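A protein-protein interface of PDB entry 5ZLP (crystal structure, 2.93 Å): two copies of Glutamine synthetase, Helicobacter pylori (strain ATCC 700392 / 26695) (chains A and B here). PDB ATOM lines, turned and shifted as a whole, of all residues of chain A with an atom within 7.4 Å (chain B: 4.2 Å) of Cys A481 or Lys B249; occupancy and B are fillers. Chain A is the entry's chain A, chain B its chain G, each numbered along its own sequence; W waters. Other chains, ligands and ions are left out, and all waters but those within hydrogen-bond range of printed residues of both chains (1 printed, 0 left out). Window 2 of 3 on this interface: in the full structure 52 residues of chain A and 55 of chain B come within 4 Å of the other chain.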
ATOM      1  N   PHE A 475      33.539   1.644 -18.804  1.00  0.00           N
ATOM      2  CA  PHE A 475      32.091   1.547 -18.961  1.00  0.00           C
ATOM      3  C   PHE A 475      31.728   0.949 -20.302  1.00  0.00           C
ATOM      4  O   PHE A 475      30.685   0.303 -20.428  1.00  0.00           O
ATOM      5  CB  PHE A 475      31.444   2.920 -18.752  1.00  0.00           C
ATOM      6  CG  PHE A 475      31.391   3.319 -17.311  1.00  0.00           C
ATOM      7  CD1 PHE A 475      32.530   3.747 -16.660  1.00  0.00           C
ATOM      8  CD2 PHE A 475      30.226   3.198 -16.590  1.00  0.00           C
ATOM      9  CE1 PHE A 475      32.488   4.071 -15.319  1.00  0.00           C
ATOM     10  CE2 PHE A 475      30.177   3.522 -15.270  1.00  0.00           C
ATOM     11  CZ  PHE A 475      31.302   3.950 -14.626  1.00  0.00           C
ATOM     12  N   ILE A 476      32.606   1.097 -21.288  1.00  0.00           N
ATOM     13  CA  ILE A 476      32.399   0.410 -22.550  1.00  0.00           C
ATOM     14  C   ILE A 476      32.599  -1.090 -22.374  1.00  0.00           C
ATOM     15  O   ILE A 476      31.877  -1.904 -22.960  1.00  0.00           O
ATOM     16  CB  ILE A 476      33.345   0.991 -23.611  1.00  0.00           C
ATOM     17  CG1 ILE A 476      32.977   2.438 -23.936  1.00  0.00           C
ATOM     18  CG2 ILE A 476      33.315   0.148 -24.852  1.00  0.00           C
ATOM     19  CD1 ILE A 476      33.868   3.052 -25.010  1.00  0.00           C
ATOM     20  N   THR A 477      33.582  -1.474 -21.562  1.00  0.00           N
ATOM     21  CA  THR A 477      34.046  -2.847 -21.465  1.00  0.00           C
ATOM     22  C   THR A 477      33.282  -3.652 -20.456  1.00  0.00           C
ATOM     23  O   THR A 477      33.163  -4.871 -20.605  1.00  0.00           O
ATOM     24  CB  THR A 477      35.500  -2.890 -21.020  1.00  0.00           C
ATOM     25  OG1 THR A 477      36.067  -1.584 -21.151  1.00  0.00           O
ATOM     26  CG2 THR A 477      36.272  -3.918 -21.843  1.00  0.00           C
ATOM     27  N   THR A 478      32.806  -3.002 -19.413  1.00  0.00           N
ATOM     28  CA  THR A 478      32.382  -3.712 -18.236  1.00  0.00           C
ATOM     29  C   THR A 478      30.991  -3.341 -17.791  1.00  0.00           C
ATOM     30  O   THR A 478      30.473  -3.989 -16.880  1.00  0.00           O
ATOM     31  CB  THR A 478      33.395  -3.479 -17.097  1.00  0.00           C
ATOM     32  OG1 THR A 478      34.694  -3.823 -17.582  1.00  0.00           O
ATOM     33  CG2 THR A 478      33.131  -4.350 -15.891  1.00  0.00           C
ATOM     34  N   TYR A 479      30.342  -2.362 -18.416  1.00  0.00           N
ATOM     35  CA  TYR A 479      28.986  -2.052 -17.979  1.00  0.00           C
ATOM     36  C   TYR A 479      28.071  -3.266 -18.120  1.00  0.00           C
ATOM     37  O   TYR A 479      27.251  -3.535 -17.243  1.00  0.00           O
ATOM     38  CB  TYR A 479      28.435  -0.856 -18.736  1.00  0.00           C
ATOM     39  CG  TYR A 479      27.149  -0.306 -18.159  1.00  0.00           C
ATOM     40  CD1 TYR A 479      27.147   0.448 -16.981  1.00  0.00           C
ATOM     41  CD2 TYR A 479      25.928  -0.511 -18.814  1.00  0.00           C
ATOM     42  CE1 TYR A 479      25.959   0.977 -16.472  1.00  0.00           C
ATOM     43  CE2 TYR A 479      24.739   0.022 -18.318  1.00  0.00           C
ATOM     44  CZ  TYR A 479      24.755   0.755 -17.149  1.00  0.00           C
ATOM     45  OH  TYR A 479      23.562   1.248 -16.660  1.00  0.00           O
ATOM     46  N   SER A 480      28.237  -4.057 -19.169  1.00  0.00           N
ATOM     47  CA  SER A 480      27.331  -5.179 -19.373  1.00  0.00           C
ATOM     48  C   SER A 480      27.867  -6.507 -18.861  1.00  0.00           C
ATOM     49  O   SER A 480      27.114  -7.488 -18.849  1.00  0.00           O
ATOM     50  CB  SER A 480      26.960  -5.290 -20.852  1.00  0.00           C
ATOM     51  OG  SER A 480      26.328  -4.077 -21.241  1.00  0.00           O
ATOM     52  N   CYS A 481      29.125  -6.565 -18.444  1.00  0.00           N
ATOM     53  CA  CYS A 481      29.613  -7.688 -17.669  1.00  0.00           C
ATOM     54  C   CYS A 481      28.609  -8.071 -16.542  1.00  0.00           C
ATOM     55  O   CYS A 481      27.940  -9.111 -16.559  1.00  0.00           O
ATOM     56  CB  CYS A 481      30.924  -7.326 -17.032  1.00  0.00           C
ATOM     57  SG  CYS A 481      30.517  -6.696 -15.368  1.00  0.00           S
ATOM     58  N   VAL B 245      24.338 -17.892 -12.277  1.00  0.00           N
ATOM     59  CA  VAL B 245      24.778 -16.498 -12.229  1.00  0.00           C
ATOM     60  C   VAL B 245      24.405 -15.798 -13.528  1.00  0.00           C
ATOM     61  O   VAL B 245      23.766 -14.742 -13.517  1.00  0.00           O
ATOM     62  CB  VAL B 245      26.288 -16.390 -11.932  1.00  0.00           C
ATOM     63  CG1 VAL B 245      26.781 -14.964 -12.155  1.00  0.00           C
ATOM     64  CG2 VAL B 245      26.594 -16.809 -10.514  1.00  0.00           C
ATOM     65  N   GLN B 246      24.781 -16.389 -14.668  1.00  0.00           N
ATOM     66  CA  GLN B 246      24.342 -15.860 -15.952  1.00  0.00           C
ATOM     67  C   GLN B 246      22.831 -15.761 -15.980  1.00  0.00           C
ATOM     68  O   GLN B 246      22.264 -14.717 -16.322  1.00  0.00           O
ATOM     69  CB  GLN B 246      24.827 -16.752 -17.098  1.00  0.00           C
ATOM     70  CG  GLN B 246      26.325 -16.975 -17.159  1.00  0.00           C
ATOM     71  CD  GLN B 246      27.049 -15.986 -18.062  1.00  0.00           C
ATOM     72  OE1 GLN B 246      27.703 -16.393 -19.027  1.00  0.00           O
ATOM     73  NE2 GLN B 246      26.954 -14.685 -17.742  1.00  0.00           N
ATOM     74  N   LYS B 247      22.162 -16.849 -15.606  1.00  0.00           N
ATOM     75  CA  LYS B 247      20.699 -16.891 -15.599  1.00  0.00           C
ATOM     76  C   LYS B 247      20.098 -15.780 -14.729  1.00  0.00           C
ATOM     77  O   LYS B 247      19.035 -15.243 -15.061  1.00  0.00           O
ATOM     78  CB  LYS B 247      20.259 -18.285 -15.138  1.00  0.00           C
ATOM     79  CG  LYS B 247      18.824 -18.639 -15.356  1.00  0.00           C
ATOM     80  CD  LYS B 247      18.484 -19.927 -14.616  1.00  0.00           C
ATOM     81  CE  LYS B 247      18.369 -21.105 -15.549  1.00  0.00           C
ATOM     82  NZ  LYS B 247      17.634 -22.212 -14.892  1.00  0.00           N
ATOM     83  N   LEU B 248      20.780 -15.412 -13.629  1.00  0.00           N
ATOM     84  CA  LEU B 248      20.384 -14.252 -12.833  1.00  0.00           C
ATOM     85  C   LEU B 248      20.743 -12.941 -13.527  1.00  0.00           C
ATOM     86  O   LEU B 248      19.938 -12.003 -13.544  1.00  0.00           O
ATOM     87  CB  LEU B 248      21.049 -14.304 -11.465  1.00  0.00           C
ATOM     88  CG  LEU B 248      20.761 -13.138 -10.523  1.00  0.00           C
ATOM     89  CD1 LEU B 248      19.899 -13.669  -9.411  1.00  0.00           C
ATOM     90  CD2 LEU B 248      22.055 -12.502  -9.992  1.00  0.00           C
ATOM     91  N   LYS B 249      21.968 -12.834 -14.059  1.00  0.00           N
ATOM     92  CA  LYS B 249      22.386 -11.612 -14.741  1.00  0.00           C
ATOM     93  C   LYS B 249      21.422 -11.255 -15.874  1.00  0.00           C
ATOM     94  O   LYS B 249      21.066 -10.087 -16.083  1.00  0.00           O
ATOM     95  CB  LYS B 249      23.801 -11.800 -15.302  1.00  0.00           C
ATOM     96  CG  LYS B 249      24.987 -11.545 -14.382  1.00  0.00           C
ATOM     97  CD  LYS B 249      26.290 -11.610 -15.203  1.00  0.00           C
ATOM     98  CE  LYS B 249      27.570 -11.611 -14.378  1.00  0.00           C
ATOM     99  NZ  LYS B 249      28.700 -11.988 -15.270  1.00  0.00           N
ATOM    100  N   TYR B 250      21.024 -12.250 -16.644  1.00  0.00           N
ATOM    101  CA  TYR B 250      20.087 -11.998 -17.717  1.00  0.00           C
ATOM    102  C   TYR B 250      18.782 -11.412 -17.161  1.00  0.00           C
ATOM    103  O   TYR B 250      18.318 -10.351 -17.603  1.00  0.00           O
ATOM    104  CB  TYR B 250      19.883 -13.312 -18.478  1.00  0.00           C
ATOM    105  CG  TYR B 250      18.933 -13.220 -19.622  1.00  0.00           C
ATOM    106  CD1 TYR B 250      19.127 -12.281 -20.629  1.00  0.00           C
ATOM    107  CD2 TYR B 250      17.826 -14.074 -19.695  1.00  0.00           C
ATOM    108  CE1 TYR B 250      18.249 -12.182 -21.683  1.00  0.00           C
ATOM    109  CE2 TYR B 250      16.935 -13.991 -20.743  1.00  0.00           C
ATOM    110  CZ  TYR B 250      17.152 -13.041 -21.740  1.00  0.00           C
ATOM    111  OH  TYR B 250      16.266 -12.956 -22.799  1.00  0.00           O
ATOM    112  N   VAL B 251      18.224 -12.051 -16.127  1.00  0.00           N
ATOM    113  CA  VAL B 251      16.922 -11.638 -15.619  1.00  0.00           C
ATOM    114  C   VAL B 251      16.959 -10.210 -15.091  1.00  0.00           C
ATOM    115  O   VAL B 251      16.046  -9.416 -15.338  1.00  0.00           O
ATOM    116  CB  VAL B 251      16.430 -12.643 -14.567  1.00  0.00           C
ATOM    117  CG1 VAL B 251      15.217 -12.100 -13.806  1.00  0.00           C
ATOM    118  CG2 VAL B 251      16.099 -13.948 -15.275  1.00  0.00           C
ATOM    119  N   VAL B 252      18.019  -9.847 -14.386  1.00  0.00           N
ATOM    120  CA  VAL B 252      18.117  -8.492 -13.858  1.00  0.00           C
ATOM    121  C   VAL B 252      18.314  -7.479 -14.984  1.00  0.00           C
ATOM    122  O   VAL B 252      17.667  -6.422 -15.004  1.00  0.00           O
ATOM    123  CB  VAL B 252      19.238  -8.413 -12.807  1.00  0.00           C
ATOM    124  CG1 VAL B 252      19.531  -6.954 -12.443  1.00  0.00           C
ATOM    125  CG2 VAL B 252      18.845  -9.177 -11.578  1.00  0.00           C
ATOM    126  N   LYS B 253      19.198  -7.774 -15.948  1.00  0.00           N
ATOM    127  CA  LYS B 253      19.427  -6.809 -17.024  1.00  0.00           C
ATOM    128  C   LYS B 253      18.200  -6.655 -17.917  1.00  0.00           C
ATOM    129  O   LYS B 253      17.980  -5.591 -18.509  1.00  0.00           O
ATOM    130  CB  LYS B 253      20.647  -7.210 -17.853  1.00  0.00           C
ATOM    131  CG  LYS B 253      21.952  -6.661 -17.336  1.00  0.00           C
ATOM    132  CD  LYS B 253      23.135  -6.980 -18.252  1.00  0.00           C
ATOM    133  CE  LYS B 253      23.601  -8.444 -18.156  1.00  0.00           C
ATOM    134  NZ  LYS B 253      25.042  -8.630 -18.553  1.00  0.00           N
ATOM    135  N   PHE B 265      26.239  -4.944 -13.628  1.00  0.00           N
ATOM    136  CA  PHE B 265      26.882  -5.678 -12.559  1.00  0.00           C
ATOM    137  C   PHE B 265      28.331  -5.264 -12.375  1.00  0.00           C
ATOM    138  O   PHE B 265      29.034  -5.888 -11.583  1.00  0.00           O
ATOM    139  CB  PHE B 265      26.777  -7.174 -12.809  1.00  0.00           C
ATOM    140  CG  PHE B 265      25.412  -7.730 -12.575  1.00  0.00           C
ATOM    141  CD1 PHE B 265      24.401  -7.507 -13.470  1.00  0.00           C
ATOM    142  CD2 PHE B 265      25.147  -8.486 -11.469  1.00  0.00           C
ATOM    143  CE1 PHE B 265      23.170  -8.028 -13.268  1.00  0.00           C
ATOM    144  CE2 PHE B 265      23.906  -9.003 -11.250  1.00  0.00           C
ATOM    145  CZ  PHE B 265      22.922  -8.776 -12.146  1.00  0.00           C
ATOM    146  N   MET B 266      28.778  -4.200 -13.043  1.00  0.00           N
ATOM    147  CA  MET B 266      30.177  -3.798 -12.955  1.00  0.00           C
ATOM    148  C   MET B 266      30.576  -3.470 -11.510  1.00  0.00           C
ATOM    149  O   MET B 266      29.737  -3.019 -10.724  1.00  0.00           O
ATOM    150  CB  MET B 266      30.460  -2.616 -13.890  1.00  0.00           C
ATOM    151  CG  MET B 266      29.698  -1.345 -13.670  1.00  0.00           C
ATOM    152  SD  MET B 266      30.203  -0.038 -14.849  1.00  0.00           S
ATOM    153  CE  MET B 266      31.858   0.380 -14.319  1.00  0.00           C
ATOM    154  N   SER B 373      31.687  -9.392 -10.205  1.00  0.00           N
ATOM    155  CA  SER B 373      30.882  -9.914 -11.285  1.00  0.00           C
ATOM    156  C   SER B 373      31.406  -9.517 -12.644  1.00  0.00           C
ATOM    157  O   SER B 373      30.737  -9.787 -13.640  1.00  0.00           O
ATOM    158  CB  SER B 373      29.441  -9.444 -11.135  1.00  0.00           C
ATOM    159  OG  SER B 373      28.973  -9.746  -9.839  1.00  0.00           O
ATOM    160  N   SER B 374      32.551  -8.840 -12.700  1.00  0.00           N
ATOM    161  CA  SER B 374      33.278  -8.715 -13.954  1.00  0.00           C
ATOM    162  C   SER B 374      33.882 -10.049 -14.344  1.00  0.00           C
ATOM    163  O   SER B 374      34.142 -10.293 -15.533  1.00  0.00           O
ATOM    164  CB  SER B 374      34.371  -7.660 -13.829  1.00  0.00           C
ATOM    165  OG  SER B 374      35.372  -8.098 -12.931  1.00  0.00           O
ATOM    166  N   SER B 375      34.080 -10.920 -13.361  1.00  0.00           N
ATOM    167  CA  SER B 375      34.629 -12.227 -13.619  1.00  0.00           C
ATOM    168  C   SER B 375      33.669 -13.073 -14.439  1.00  0.00           C
ATOM    169  O   SER B 375      32.460 -12.829 -14.508  1.00  0.00           O
ATOM    170  CB  SER B 375      34.928 -12.944 -12.312  1.00  0.00           C
ATOM    171  OG  SER B 375      33.743 -13.143 -11.579  1.00  0.00           O
HETATM  172  O   HOH W   1      26.890 -10.160 -20.817  1.00  0.00           O
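NZ of Lys B249 is in hydrogen-bond range of O of Cys A481 (3.2 Å).
The side-chain sulfur (SG) of Cys A481 sits at hydrogen-bond distance from the backbone carbonyl oxygen (O) of Ser B373, at 3.5 Å.
The side-chain amino group of Lys B253 sits close to the backbone carbonyl oxygen of Ser A480 (2.4 Å).
The backbone carbonyl oxygen (O) of Thr A478 is in hydrogen-bond range of the side-chain sulfur (SG) of Cys A481 (3.1 Å).
The backbone carbonyl oxygen (O) of Ser B373 lies within hydrogen-bond range of the side-chain amino group (NZ) of Lys B249 (3.4 Å).
Among the printed residues, pairs that only touch across the chains: Thr A478 with Met B266, Cys A481 with Lys B253, Phe A475 with Met B266, Cys A481 with Ser B374, Tyr A479 with Met B266, Cys A481 with Met B266 and Cys A481 with Phe B265.
Cys A481 touches six residues of chain B.
Of the printed residues of chain A, Lys B249 touches Cys A481.
Of the printed residues of chain A, Met B266 touches Phe A475 (3.6 Å), Thr A478 (3.3 Å), Tyr A479 (3.8 Å) and Cys A481 (3.8 Å).
Of the printed residues of chain A, Phe B265 touches Cys A481.
Thr A477 touches none of the printed residues of chain B.
The nearest residue of chain A that does not touch Lys B249 is Ser A480 (5.6 Å).
The nearest printed residue of chain A that does not touch Met B266 is Ser A480 (5.9 Å).
Hydrophobic or aromatic side chains of chain B within 4 Å of the printed part of chain A: Met B266.
Hydrophobic or aromatic side chains of chain A that line the printed part of chain B: Phe A475 and Tyr A479.
Among the printed residues, no Asp or Glu carboxylate lies within 4 Å of a Lys or Arg side-chain nitrogen of the other chain.
No position is printed for both chains.
Water W1 lies within hydrogen-bond range of NZ of Lys B253 (3.3 Å) and O of Ser A480 (3.3 Å).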
